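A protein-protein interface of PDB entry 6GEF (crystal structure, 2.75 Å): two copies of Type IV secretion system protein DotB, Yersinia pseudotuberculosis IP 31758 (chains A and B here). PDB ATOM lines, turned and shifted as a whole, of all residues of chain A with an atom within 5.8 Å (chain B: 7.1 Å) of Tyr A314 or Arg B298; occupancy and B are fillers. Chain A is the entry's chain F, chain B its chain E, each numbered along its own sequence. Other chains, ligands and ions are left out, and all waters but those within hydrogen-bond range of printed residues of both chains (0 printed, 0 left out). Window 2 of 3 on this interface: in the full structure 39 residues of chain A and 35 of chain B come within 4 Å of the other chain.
O of Ala B295 is in hydrogen-bond range of OH of Tyr A314 (3.2 Å). The side-chain carboxylate (OE2) of Glu A351 lies within salt-bridge range of the guanidinium group (NH1) of Arg B298, 3.5 Å away. OH of Tyr A314 lies close to N of Arg B299. NH1 of Arg B299 is in salt-bridge range of OE2 of Glu A318, 3.2 Å away. O of Ser B302 lies within hydrogen-bond range of N of Ala A311 (3.4 Å). The guanidinium group (NH1) of Arg B303 is in hydrogen-bond range of the backbone carbonyl oxygen (O) of Ala A311, at 3.2 Å. The guanidinium group (NH1) of Arg B303 is in salt-bridge range of the side-chain carboxylate (OD1) of Asp A315 (2.5 Å).
The side-chain hydroxyl (OG) of Ser B290 lies within hydrogen-bond range of the backbone carbonyl oxygen (O) of Ala B295 (3.1 Å). The backbone NH (N) of Ala B295 lies within hydrogen-bond range of the side-chain amide oxygen (OD1) of Asn B292 (3.0 Å). OG of Ser B302 is in hydrogen-bond range of O of Arg B299 (2.4 Å). The guanidinium group (NH1) of Arg B303 lies within hydrogen-bond range of the side-chain hydroxyl (OG) of Ser B302. O of Asp A315 is in hydrogen-bond range of OG1 of Thr A319 (2.7 Å).
Tyr A314 touches Arg B298 (CE2 to CG, 3.6 Å). Tyr A314 touches Ser B302. Tyr A314 touches Arg B303.
Printed residues of chain B within 4 Å of Ala A311: Ser B302 (3.4 Å) and Arg B303 (3.2 Å). Tyr A314 touches just these residues of chain B: Ala B295, Arg B298, Arg B299, Ser B302 and Arg B303. Of the printed residues of chain B, Asp A315 touches Arg B303 (2.4 Å). Printed residues of chain B within 4 Å of Glu A318: Arg B299 (3.2 Å). Ser B290 touches none of the printed residues of chain A. Cys B293 touches none of the printed residues of chain A. Arg B298 touches just these residues of chain A: Tyr A314 and Glu A351. Of the printed residues of chain A, Arg B299 touches Tyr A314 and Glu A318. The nearest residue of chain A that does not touch Arg B298 is Leu A354 (4.2 Å).
Of the 21 printed residues of chain B, 5 touch a printed residue of chain A. Printed residues of chain B that touch a printed residue of chain A: Ala B295, Arg B298, Arg B299, Ser B302 and Arg B303. Along chain B the printed residues that touch a printed residue of chain A span positions 295 to 303. Printed residues of chain A that touch a printed residue of chain B: Ala A311, Tyr A314, Asp A315, Glu A318 and Glu A351. Hydrophobic or aromatic side chains of chain A that line the printed part of chain B: Ala A311 and Tyr A314. Among the printed residues, 10 pairs touch across the chains. Among the printed residues, Asp or Glu carboxylates within 4 Å of a Lys or Arg side-chain nitrogen of the other chain: Asp A315 with Arg B303 (2.4 Å), Glu A318 with Arg B299 (3.2 Å) and Glu A351 with Arg B298 (3.5 Å).
1 position is printed for both chains. Of the 10 pairs that touch across the chains among the printed residues, none has its exchanged pair printed and touching as well.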
ATOM      1  N   ARG A 309       9.572   4.517 -17.497  1.00  0.00           N
ATOM      2  CA  ARG A 309       9.701   4.917 -16.094  1.00  0.00           C
ATOM      3  C   ARG A 309      10.811   5.960 -15.865  1.00  0.00           C
ATOM      4  O   ARG A 309      10.783   6.676 -14.874  1.00  0.00           O
ATOM      5  CB  ARG A 309       9.966   3.696 -15.202  1.00  0.00           C
ATOM      6  CG  ARG A 309      10.314   4.055 -13.784  1.00  0.00           C
ATOM      7  CD  ARG A 309      10.595   2.800 -12.973  1.00  0.00           C
ATOM      8  NE  ARG A 309       9.425   1.979 -12.851  1.00  0.00           N
ATOM      9  CZ  ARG A 309       9.425   0.628 -12.829  1.00  0.00           C
ATOM     10  NH1 ARG A 309      10.545  -0.012 -12.994  1.00  0.00           N
ATOM     11  NH2 ARG A 309       8.286  -0.037 -12.687  1.00  0.00           N
ATOM     12  N   GLY A 310      11.785   6.032 -16.775  1.00  0.00           N
ATOM     13  CA  GLY A 310      12.770   7.077 -16.741  1.00  0.00           C
ATOM     14  C   GLY A 310      12.247   8.474 -16.934  1.00  0.00           C
ATOM     15  O   GLY A 310      12.373   9.363 -16.082  1.00  0.00           O
ATOM     16  N   ALA A 311      11.574   8.666 -18.067  1.00  0.00           N
ATOM     17  CA  ALA A 311      10.750   9.878 -18.284  1.00  0.00           C
ATOM     18  C   ALA A 311       9.904  10.212 -17.061  1.00  0.00           C
ATOM     19  O   ALA A 311       9.813  11.358 -16.664  1.00  0.00           O
ATOM     20  CB  ALA A 311       9.912   9.702 -19.523  1.00  0.00           C
ATOM     21  N   ALA A 312       9.301   9.248 -16.471  1.00  0.00           N
ATOM     22  CA  ALA A 312       8.432   9.484 -15.302  1.00  0.00           C
ATOM     23  C   ALA A 312       9.234   9.961 -14.132  1.00  0.00           C
ATOM     24  O   ALA A 312       8.770  10.843 -13.386  1.00  0.00           O
ATOM     25  CB  ALA A 312       7.603   8.215 -14.937  1.00  0.00           C
ATOM     26  N   ILE A 313      10.405   9.382 -13.905  1.00  0.00           N
ATOM     27  CA  ILE A 313      11.257   9.810 -12.791  1.00  0.00           C
ATOM     28  C   ILE A 313      11.706  11.279 -13.015  1.00  0.00           C
ATOM     29  O   ILE A 313      11.654  12.101 -12.091  1.00  0.00           O
ATOM     30  CB  ILE A 313      12.462   8.889 -12.622  1.00  0.00           C
ATOM     31  CG1 ILE A 313      12.003   7.474 -12.254  1.00  0.00           C
ATOM     32  CG2 ILE A 313      13.405   9.462 -11.561  1.00  0.00           C
ATOM     33  CD1 ILE A 313      13.063   6.559 -11.673  1.00  0.00           C
ATOM     34  N   TYR A 314      12.126  11.601 -14.250  1.00  0.00           N
ATOM     35  CA  TYR A 314      12.502  12.958 -14.550  1.00  0.00           C
ATOM     36  C   TYR A 314      11.360  13.937 -14.343  1.00  0.00           C
ATOM     37  O   TYR A 314      11.518  14.995 -13.740  1.00  0.00           O
ATOM     38  CB  TYR A 314      13.075  13.052 -15.982  1.00  0.00           C
ATOM     39  CG  TYR A 314      13.395  14.485 -16.414  1.00  0.00           C
ATOM     40  CD1 TYR A 314      12.384  15.320 -16.859  1.00  0.00           C
ATOM     41  CD2 TYR A 314      14.654  14.995 -16.353  1.00  0.00           C
ATOM     42  CE1 TYR A 314      12.631  16.598 -17.266  1.00  0.00           C
ATOM     43  CE2 TYR A 314      14.923  16.303 -16.709  1.00  0.00           C
ATOM     44  CZ  TYR A 314      13.905  17.118 -17.117  1.00  0.00           C
ATOM     45  OH  TYR A 314      14.194  18.422 -17.495  1.00  0.00           O
ATOM     46  N   ASP A 315      10.215  13.624 -14.871  1.00  0.00           N
ATOM     47  CA  ASP A 315       9.010  14.468 -14.659  1.00  0.00           C
ATOM     48  C   ASP A 315       8.752  14.653 -13.177  1.00  0.00           C
ATOM     49  O   ASP A 315       8.490  15.763 -12.716  1.00  0.00           O
ATOM     50  CB  ASP A 315       7.803  13.873 -15.368  1.00  0.00           C
ATOM     51  CG  ASP A 315       8.018  13.679 -16.845  1.00  0.00           C
ATOM     52  OD1 ASP A 315       9.149  13.956 -17.338  1.00  0.00           O
ATOM     53  OD2 ASP A 315       7.131  13.215 -17.564  1.00  0.00           O
ATOM     54  N   LEU A 316       8.791  13.563 -12.405  1.00  0.00           N
ATOM     55  CA  LEU A 316       8.467  13.642 -10.996  1.00  0.00           C
ATOM     56  C   LEU A 316       9.450  14.520 -10.222  1.00  0.00           C
ATOM     57  O   LEU A 316       9.063  15.367  -9.430  1.00  0.00           O
ATOM     58  CB  LEU A 316       8.394  12.242 -10.385  1.00  0.00           C
ATOM     59  CG  LEU A 316       7.879  12.185  -8.942  1.00  0.00           C
ATOM     60  CD1 LEU A 316       6.566  12.932  -8.752  1.00  0.00           C
ATOM     61  CD2 LEU A 316       7.698  10.739  -8.493  1.00  0.00           C
ATOM     62  N   VAL A 317      10.738  14.325 -10.468  1.00  0.00           N
ATOM     63  CA  VAL A 317      11.763  15.145  -9.810  1.00  0.00           C
ATOM     64  C   VAL A 317      11.668  16.620 -10.247  1.00  0.00           C
ATOM     65  O   VAL A 317      11.822  17.515  -9.429  1.00  0.00           O
ATOM     66  CB  VAL A 317      13.168  14.575 -10.061  1.00  0.00           C
ATOM     67  CG1 VAL A 317      14.218  15.462  -9.443  1.00  0.00           C
ATOM     68  CG2 VAL A 317      13.285  13.182  -9.482  1.00  0.00           C
ATOM     69  N   GLU A 318      11.366  16.849 -11.504  1.00  0.00           N
ATOM     70  CA  GLU A 318      11.411  18.194 -12.056  1.00  0.00           C
ATOM     71  C   GLU A 318      10.164  19.000 -11.767  1.00  0.00           C
ATOM     72  O   GLU A 318      10.216  20.225 -11.790  1.00  0.00           O
ATOM     73  CB  GLU A 318      11.667  18.132 -13.567  1.00  0.00           C
ATOM     74  CG  GLU A 318      11.724  19.452 -14.262  1.00  0.00           C
ATOM     75  CD  GLU A 318      10.345  19.833 -14.870  1.00  0.00           C
ATOM     76  OE1 GLU A 318       9.729  20.871 -14.477  1.00  0.00           O
ATOM     77  OE2 GLU A 318       9.886  19.072 -15.759  1.00  0.00           O
ATOM     78  N   THR A 319       9.036  18.348 -11.509  1.00  0.00           N
ATOM     79  CA  THR A 319       7.806  19.036 -11.155  1.00  0.00           C
ATOM     80  C   THR A 319       7.586  19.130  -9.651  1.00  0.00           C
ATOM     81  O   THR A 319       6.869  20.028  -9.197  1.00  0.00           O
ATOM     82  CB  THR A 319       6.589  18.350 -11.803  1.00  0.00           C
ATOM     83  OG1 THR A 319       6.498  17.010 -11.354  1.00  0.00           O
ATOM     84  CG2 THR A 319       6.698  18.373 -13.311  1.00  0.00           C
ATOM     85  N   GLU A 351      18.427  19.088  -8.945  1.00  0.00           N
ATOM     86  CA  GLU A 351      19.582  18.819  -9.828  1.00  0.00           C
ATOM     87  C   GLU A 351      20.385  17.661  -9.294  1.00  0.00           C
ATOM     88  O   GLU A 351      20.874  16.821 -10.067  1.00  0.00           O
ATOM     89  CB  GLU A 351      20.418  20.070  -9.999  1.00  0.00           C
ATOM     90  CG  GLU A 351      21.543  19.899 -11.003  1.00  0.00           C
ATOM     91  CD  GLU A 351      21.508  20.913 -12.136  1.00  0.00           C
ATOM     92  OE1 GLU A 351      20.569  21.789 -12.225  1.00  0.00           O
ATOM     93  OE2 GLU A 351      22.469  20.807 -12.944  1.00  0.00           O
ATOM     94  N   LEU A 354      18.664  14.590 -10.265  1.00  0.00           N
ATOM     95  CA  LEU A 354      18.627  14.348 -11.707  1.00  0.00           C
ATOM     96  C   LEU A 354      19.862  13.663 -12.213  1.00  0.00           C
ATOM     97  O   LEU A 354      19.771  12.886 -13.175  1.00  0.00           O
ATOM     98  CB  LEU A 354      18.367  15.675 -12.464  1.00  0.00           C
ATOM     99  CG  LEU A 354      16.999  16.296 -12.285  1.00  0.00           C
ATOM    100  CD1 LEU A 354      16.989  17.641 -13.026  1.00  0.00           C
ATOM    101  CD2 LEU A 354      15.872  15.393 -12.757  1.00  0.00           C
ATOM    102  N   HIS B 289       7.726  21.875 -22.626  1.00  0.00           N
ATOM    103  CA  HIS B 289       7.421  22.319 -21.257  1.00  0.00           C
ATOM    104  C   HIS B 289       8.667  22.037 -20.417  1.00  0.00           C
ATOM    105  O   HIS B 289       8.743  21.119 -19.599  1.00  0.00           O
ATOM    106  CB  HIS B 289       6.180  21.601 -20.721  1.00  0.00           C
ATOM    107  CG  HIS B 289       4.914  22.360 -20.972  1.00  0.00           C
ATOM    108  ND1 HIS B 289       4.242  22.334 -22.166  1.00  0.00           N
ATOM    109  CD2 HIS B 289       4.171  23.144 -20.147  1.00  0.00           C
ATOM    110  CE1 HIS B 289       3.154  23.085 -22.077  1.00  0.00           C
ATOM    111  NE2 HIS B 289       3.104  23.609 -20.864  1.00  0.00           N
ATOM    112  N   SER B 290       9.640  22.928 -20.553  1.00  0.00           N
ATOM    113  CA  SER B 290      10.785  23.014 -19.667  1.00  0.00           C
ATOM    114  C   SER B 290      11.056  24.476 -19.339  1.00  0.00           C
ATOM    115  O   SER B 290      10.637  25.391 -20.073  1.00  0.00           O
ATOM    116  CB  SER B 290      12.021  22.378 -20.335  1.00  0.00           C
ATOM    117  OG  SER B 290      11.988  20.983 -20.253  1.00  0.00           O
ATOM    118  N   GLN B 291      11.819  24.681 -18.262  1.00  0.00           N
ATOM    119  CA  GLN B 291      12.076  26.035 -17.777  1.00  0.00           C
ATOM    120  C   GLN B 291      13.059  26.797 -18.672  1.00  0.00           C
ATOM    121  O   GLN B 291      12.889  27.965 -18.957  1.00  0.00           O
ATOM    122  CB  GLN B 291      12.531  26.010 -16.340  1.00  0.00           C
ATOM    123  CG  GLN B 291      12.204  27.220 -15.526  1.00  0.00           C
ATOM    124  CD  GLN B 291      12.893  27.222 -14.146  1.00  0.00           C
ATOM    125  OE1 GLN B 291      13.475  26.226 -13.683  1.00  0.00           O
ATOM    126  NE2 GLN B 291      12.835  28.353 -13.472  1.00  0.00           N
ATOM    127  N   ASN B 292      14.106  26.102 -19.111  1.00  0.00           N
ATOM    128  CA  ASN B 292      15.210  26.729 -19.833  1.00  0.00           C
ATOM    129  C   ASN B 292      15.830  25.702 -20.762  1.00  0.00           C
ATOM    130  O   ASN B 292      15.402  24.536 -20.817  1.00  0.00           O
ATOM    131  CB  ASN B 292      16.255  27.293 -18.861  1.00  0.00           C
ATOM    132  CG  ASN B 292      16.713  26.285 -17.846  1.00  0.00           C
ATOM    133  OD1 ASN B 292      17.149  25.197 -18.161  1.00  0.00           O
ATOM    134  ND2 ASN B 292      16.574  26.676 -16.561  1.00  0.00           N
ATOM    135  N   CYS B 293      16.820  26.128 -21.543  1.00  0.00           N
ATOM    136  CA  CYS B 293      17.337  25.327 -22.642  1.00  0.00           C
ATOM    137  C   CYS B 293      17.974  24.028 -22.159  1.00  0.00           C
ATOM    138  O   CYS B 293      17.554  22.943 -22.555  1.00  0.00           O
ATOM    139  CB  CYS B 293      18.329  26.138 -23.460  1.00  0.00           C
ATOM    140  SG  CYS B 293      17.806  27.813 -23.892  1.00  0.00           S
ATOM    141  N   SER B 294      18.886  24.130 -21.200  1.00  0.00           N
ATOM    142  CA  SER B 294      19.404  22.955 -20.510  1.00  0.00           C
ATOM    143  C   SER B 294      18.272  21.992 -20.115  1.00  0.00           C
ATOM    144  O   SER B 294      18.329  20.795 -20.420  1.00  0.00           O
ATOM    145  CB  SER B 294      20.186  23.363 -19.256  1.00  0.00           C
ATOM    146  OG  SER B 294      21.143  24.343 -19.590  1.00  0.00           O
ATOM    147  N   ALA B 295      17.226  22.546 -19.490  1.00  0.00           N
ATOM    148  CA  ALA B 295      16.106  21.717 -19.092  1.00  0.00           C
ATOM    149  C   ALA B 295      15.418  21.100 -20.298  1.00  0.00           C
ATOM    150  O   ALA B 295      14.922  19.967 -20.211  1.00  0.00           O
ATOM    151  CB  ALA B 295      15.121  22.531 -18.258  1.00  0.00           C
ATOM    152  N   VAL B 296      15.367  21.817 -21.419  1.00  0.00           N
ATOM    153  CA  VAL B 296      14.787  21.271 -22.644  1.00  0.00           C
ATOM    154  C   VAL B 296      15.565  20.033 -23.082  1.00  0.00           C
ATOM    155  O   VAL B 296      15.000  18.940 -23.241  1.00  0.00           O
ATOM    156  CB  VAL B 296      14.733  22.331 -23.750  1.00  0.00           C
ATOM    157  CG1 VAL B 296      14.112  21.755 -24.995  1.00  0.00           C
ATOM    158  CG2 VAL B 296      13.936  23.536 -23.278  1.00  0.00           C
ATOM    159  N   MET B 297      16.888  20.202 -23.262  1.00  0.00           N
ATOM    160  CA  MET B 297      17.720  19.086 -23.649  1.00  0.00           C
ATOM    161  C   MET B 297      17.526  17.903 -22.701  1.00  0.00           C
ATOM    162  O   MET B 297      17.177  16.790 -23.110  1.00  0.00           O
ATOM    163  CB  MET B 297      19.170  19.529 -23.706  1.00  0.00           C
ATOM    164  CG  MET B 297      19.484  20.466 -24.864  1.00  0.00           C
ATOM    165  SD  MET B 297      19.241  19.730 -26.467  1.00  0.00           S
ATOM    166  CE  MET B 297      20.309  18.289 -26.340  1.00  0.00           C
ATOM    167  N   ARG B 298      17.756  18.128 -21.419  1.00  0.00           N
ATOM    168  CA  ARG B 298      17.688  17.039 -20.439  1.00  0.00           C
ATOM    169  C   ARG B 298      16.337  16.342 -20.497  1.00  0.00           C
ATOM    170  O   ARG B 298      16.277  15.110 -20.592  1.00  0.00           O
ATOM    171  CB  ARG B 298      17.944  17.580 -19.041  1.00  0.00           C
ATOM    172  CG  ARG B 298      18.314  16.541 -18.018  1.00  0.00           C
ATOM    173  CD  ARG B 298      19.161  17.121 -16.865  1.00  0.00           C
ATOM    174  NE  ARG B 298      18.870  18.546 -16.708  1.00  0.00           N
ATOM    175  CZ  ARG B 298      19.577  19.402 -16.007  1.00  0.00           C
ATOM    176  NH1 ARG B 298      20.594  18.988 -15.255  1.00  0.00           N
ATOM    177  NH2 ARG B 298      19.208  20.689 -15.992  1.00  0.00           N
ATOM    178  N   ARG B 299      15.251  17.106 -20.496  1.00  0.00           N
ATOM    179  CA  ARG B 299      13.925  16.507 -20.568  1.00  0.00           C
ATOM    180  C   ARG B 299      13.731  15.660 -21.820  1.00  0.00           C
ATOM    181  O   ARG B 299      13.298  14.523 -21.739  1.00  0.00           O
ATOM    182  CB  ARG B 299      12.845  17.606 -20.526  1.00  0.00           C
ATOM    183  CG  ARG B 299      11.440  17.067 -20.391  1.00  0.00           C
ATOM    184  CD  ARG B 299      10.435  17.891 -21.136  1.00  0.00           C
ATOM    185  NE  ARG B 299       9.072  17.425 -20.886  1.00  0.00           N
ATOM    186  CZ  ARG B 299       8.490  17.399 -19.694  1.00  0.00           C
ATOM    187  NH1 ARG B 299       9.184  17.772 -18.582  1.00  0.00           N
ATOM    188  NH2 ARG B 299       7.232  17.011 -19.606  1.00  0.00           N
ATOM    189  N   LEU B 300      14.124  16.185 -22.967  1.00  0.00           N
ATOM    190  CA  LEU B 300      14.002  15.425 -24.213  1.00  0.00           C
ATOM    191  C   LEU B 300      14.804  14.112 -24.122  1.00  0.00           C
ATOM    192  O   LEU B 300      14.312  13.058 -24.558  1.00  0.00           O
ATOM    193  CB  LEU B 300      14.497  16.256 -25.396  1.00  0.00           C
ATOM    194  CG  LEU B 300      13.700  17.523 -25.702  1.00  0.00           C
ATOM    195  CD1 LEU B 300      14.248  18.247 -26.910  1.00  0.00           C
ATOM    196  CD2 LEU B 300      12.259  17.147 -25.919  1.00  0.00           C
ATOM    197  N   ILE B 301      16.012  14.173 -23.553  1.00  0.00           N
ATOM    198  CA  ILE B 301      16.812  12.975 -23.469  1.00  0.00           C
ATOM    199  C   ILE B 301      16.198  11.966 -22.507  1.00  0.00           C
ATOM    200  O   ILE B 301      16.306  10.755 -22.696  1.00  0.00           O
ATOM    201  CB  ILE B 301      18.280  13.319 -23.076  1.00  0.00           C
ATOM    202  CG1 ILE B 301      18.927  14.195 -24.139  1.00  0.00           C
ATOM    203  CG2 ILE B 301      19.094  12.072 -22.871  1.00  0.00           C
ATOM    204  CD1 ILE B 301      20.133  14.939 -23.611  1.00  0.00           C
ATOM    205  N   SER B 302      15.543  12.445 -21.450  1.00  0.00           N
ATOM    206  CA  SER B 302      14.955  11.543 -20.458  1.00  0.00           C
ATOM    207  C   SER B 302      13.950  10.567 -21.084  1.00  0.00           C
ATOM    208  O   SER B 302      13.780   9.458 -20.598  1.00  0.00           O
ATOM    209  CB  SER B 302      14.308  12.322 -19.327  1.00  0.00           C
ATOM    210  OG  SER B 302      13.215  13.060 -19.793  1.00  0.00           O
ATOM    211  N   ARG B 303      13.315  10.974 -22.168  1.00  0.00           N
ATOM    212  CA  ARG B 303      12.305  10.113 -22.802  1.00  0.00           C
ATOM    213  C   ARG B 303      12.867   8.808 -23.337  1.00  0.00           C
ATOM    214  O   ARG B 303      12.134   7.854 -23.497  1.00  0.00           O
ATOM    215  CB  ARG B 303      11.561  10.869 -23.904  1.00  0.00           C
ATOM    216  CG  ARG B 303      10.379  11.699 -23.397  1.00  0.00           C
ATOM    217  CD  ARG B 303      10.684  12.355 -22.063  1.00  0.00           C
ATOM    218  NE  ARG B 303       9.475  12.827 -21.421  1.00  0.00           N
ATOM    219  CZ  ARG B 303       9.381  13.157 -20.146  1.00  0.00           C
ATOM    220  NH1 ARG B 303      10.425  13.071 -19.320  1.00  0.00           N
ATOM    221  NH2 ARG B 303       8.170  13.524 -19.692  1.00  0.00           N
ATOM    222  N   LEU B 316      19.129  14.425 -31.425  1.00  0.00           N
ATOM    223  CA  LEU B 316      18.648  15.668 -30.854  1.00  0.00           C
ATOM    224  C   LEU B 316      19.602  16.819 -31.123  1.00  0.00           C
ATOM    225  O   LEU B 316      19.177  17.927 -31.433  1.00  0.00           O
ATOM    226  CB  LEU B 316      18.409  15.495 -29.350  1.00  0.00           C
ATOM    227  CG  LEU B 316      17.909  16.734 -28.588  1.00  0.00           C
ATOM    228  CD1 LEU B 316      16.582  17.189 -29.188  1.00  0.00           C
ATOM    229  CD2 LEU B 316      17.776  16.438 -27.114  1.00  0.00           C
ATOM    230  N   GLY B 360      26.066  11.916 -21.139  1.00  0.00           N
ATOM    231  CA  GLY B 360      25.524  12.389 -19.848  1.00  0.00           C
ATOM    232  C   GLY B 360      25.750  13.882 -19.591  1.00  0.00           C
ATOM    233  O   GLY B 360      24.973  14.498 -18.912  1.00  0.00           O
ATOM    234  N   VAL B 362      25.809  16.265 -21.999  1.00  0.00           N
ATOM    235  CA  VAL B 362      25.331  17.129 -23.089  1.00  0.00           C
ATOM    236  C   VAL B 362      24.522  18.322 -22.536  1.00  0.00           C
ATOM    237  O   VAL B 362      24.907  19.477 -22.656  1.00  0.00           O
ATOM    238  CB  VAL B 362      24.490  16.334 -24.085  1.00  0.00           C
ATOM    239  CG1 VAL B 362      23.314  15.668 -23.379  1.00  0.00           C
ATOM    240  CG2 VAL B 362      23.991  17.214 -25.200  1.00  0.00           C
ATOM    241  N   ALA B 363      23.471  18.001 -21.805  1.00  0.00           N
ATOM    242  CA  ALA B 363      22.676  19.015 -21.128  1.00  0.00           C
ATOM    243  C   ALA B 363      23.557  20.076 -20.466  1.00  0.00           C
ATOM    244  O   ALA B 363      23.499  21.252 -20.830  1.00  0.00           O
ATOM    245  CB  ALA B 363      21.732  18.368 -20.111  1.00  0.00           C
ATOM    246  N   SER B 364      24.376  19.652 -19.534  1.00  0.00           N
ATOM    247  CA  SER B 364      25.322  20.564 -18.887  1.00  0.00           C
ATOM    248  C   SER B 364      26.043  21.443 -19.923  1.00  0.00           C
ATOM    249  O   SER B 364      25.946  22.660 -19.905  1.00  0.00           O
ATOM    250  CB  SER B 364      26.330  19.774 -18.047  1.00  0.00           C
ATOM    251  OG  SER B 364      26.784  20.540 -16.961  1.00  0.00           O
ATOM    252  N   ARG B 367      23.959  24.228 -21.338  1.00  0.00           N
ATOM    253  CA  ARG B 367      24.041  25.318 -20.361  1.00  0.00           C
ATOM    254  C   ARG B 367      25.286  26.164 -20.595  1.00  0.00           C
ATOM    255  O   ARG B 367      25.190  27.307 -21.068  1.00  0.00           O
ATOM    256  CB  ARG B 367      24.005  24.776 -18.938  1.00  0.00           C
ATOM    257  CG  ARG B 367      23.849  25.825 -17.872  1.00  0.00           C
ATOM    258  CD  ARG B 367      22.464  26.424 -17.850  1.00  0.00           C
ATOM    259  NE  ARG B 367      21.590  25.763 -16.889  1.00  0.00           N
ATOM    260  CZ  ARG B 367      20.504  26.319 -16.344  1.00  0.00           C
ATOM    261  NH1 ARG B 367      20.146  27.563 -16.651  1.00  0.00           N
ATOM    262  NH2 ARG B 367      19.767  25.625 -15.474  1.00  0.00           N
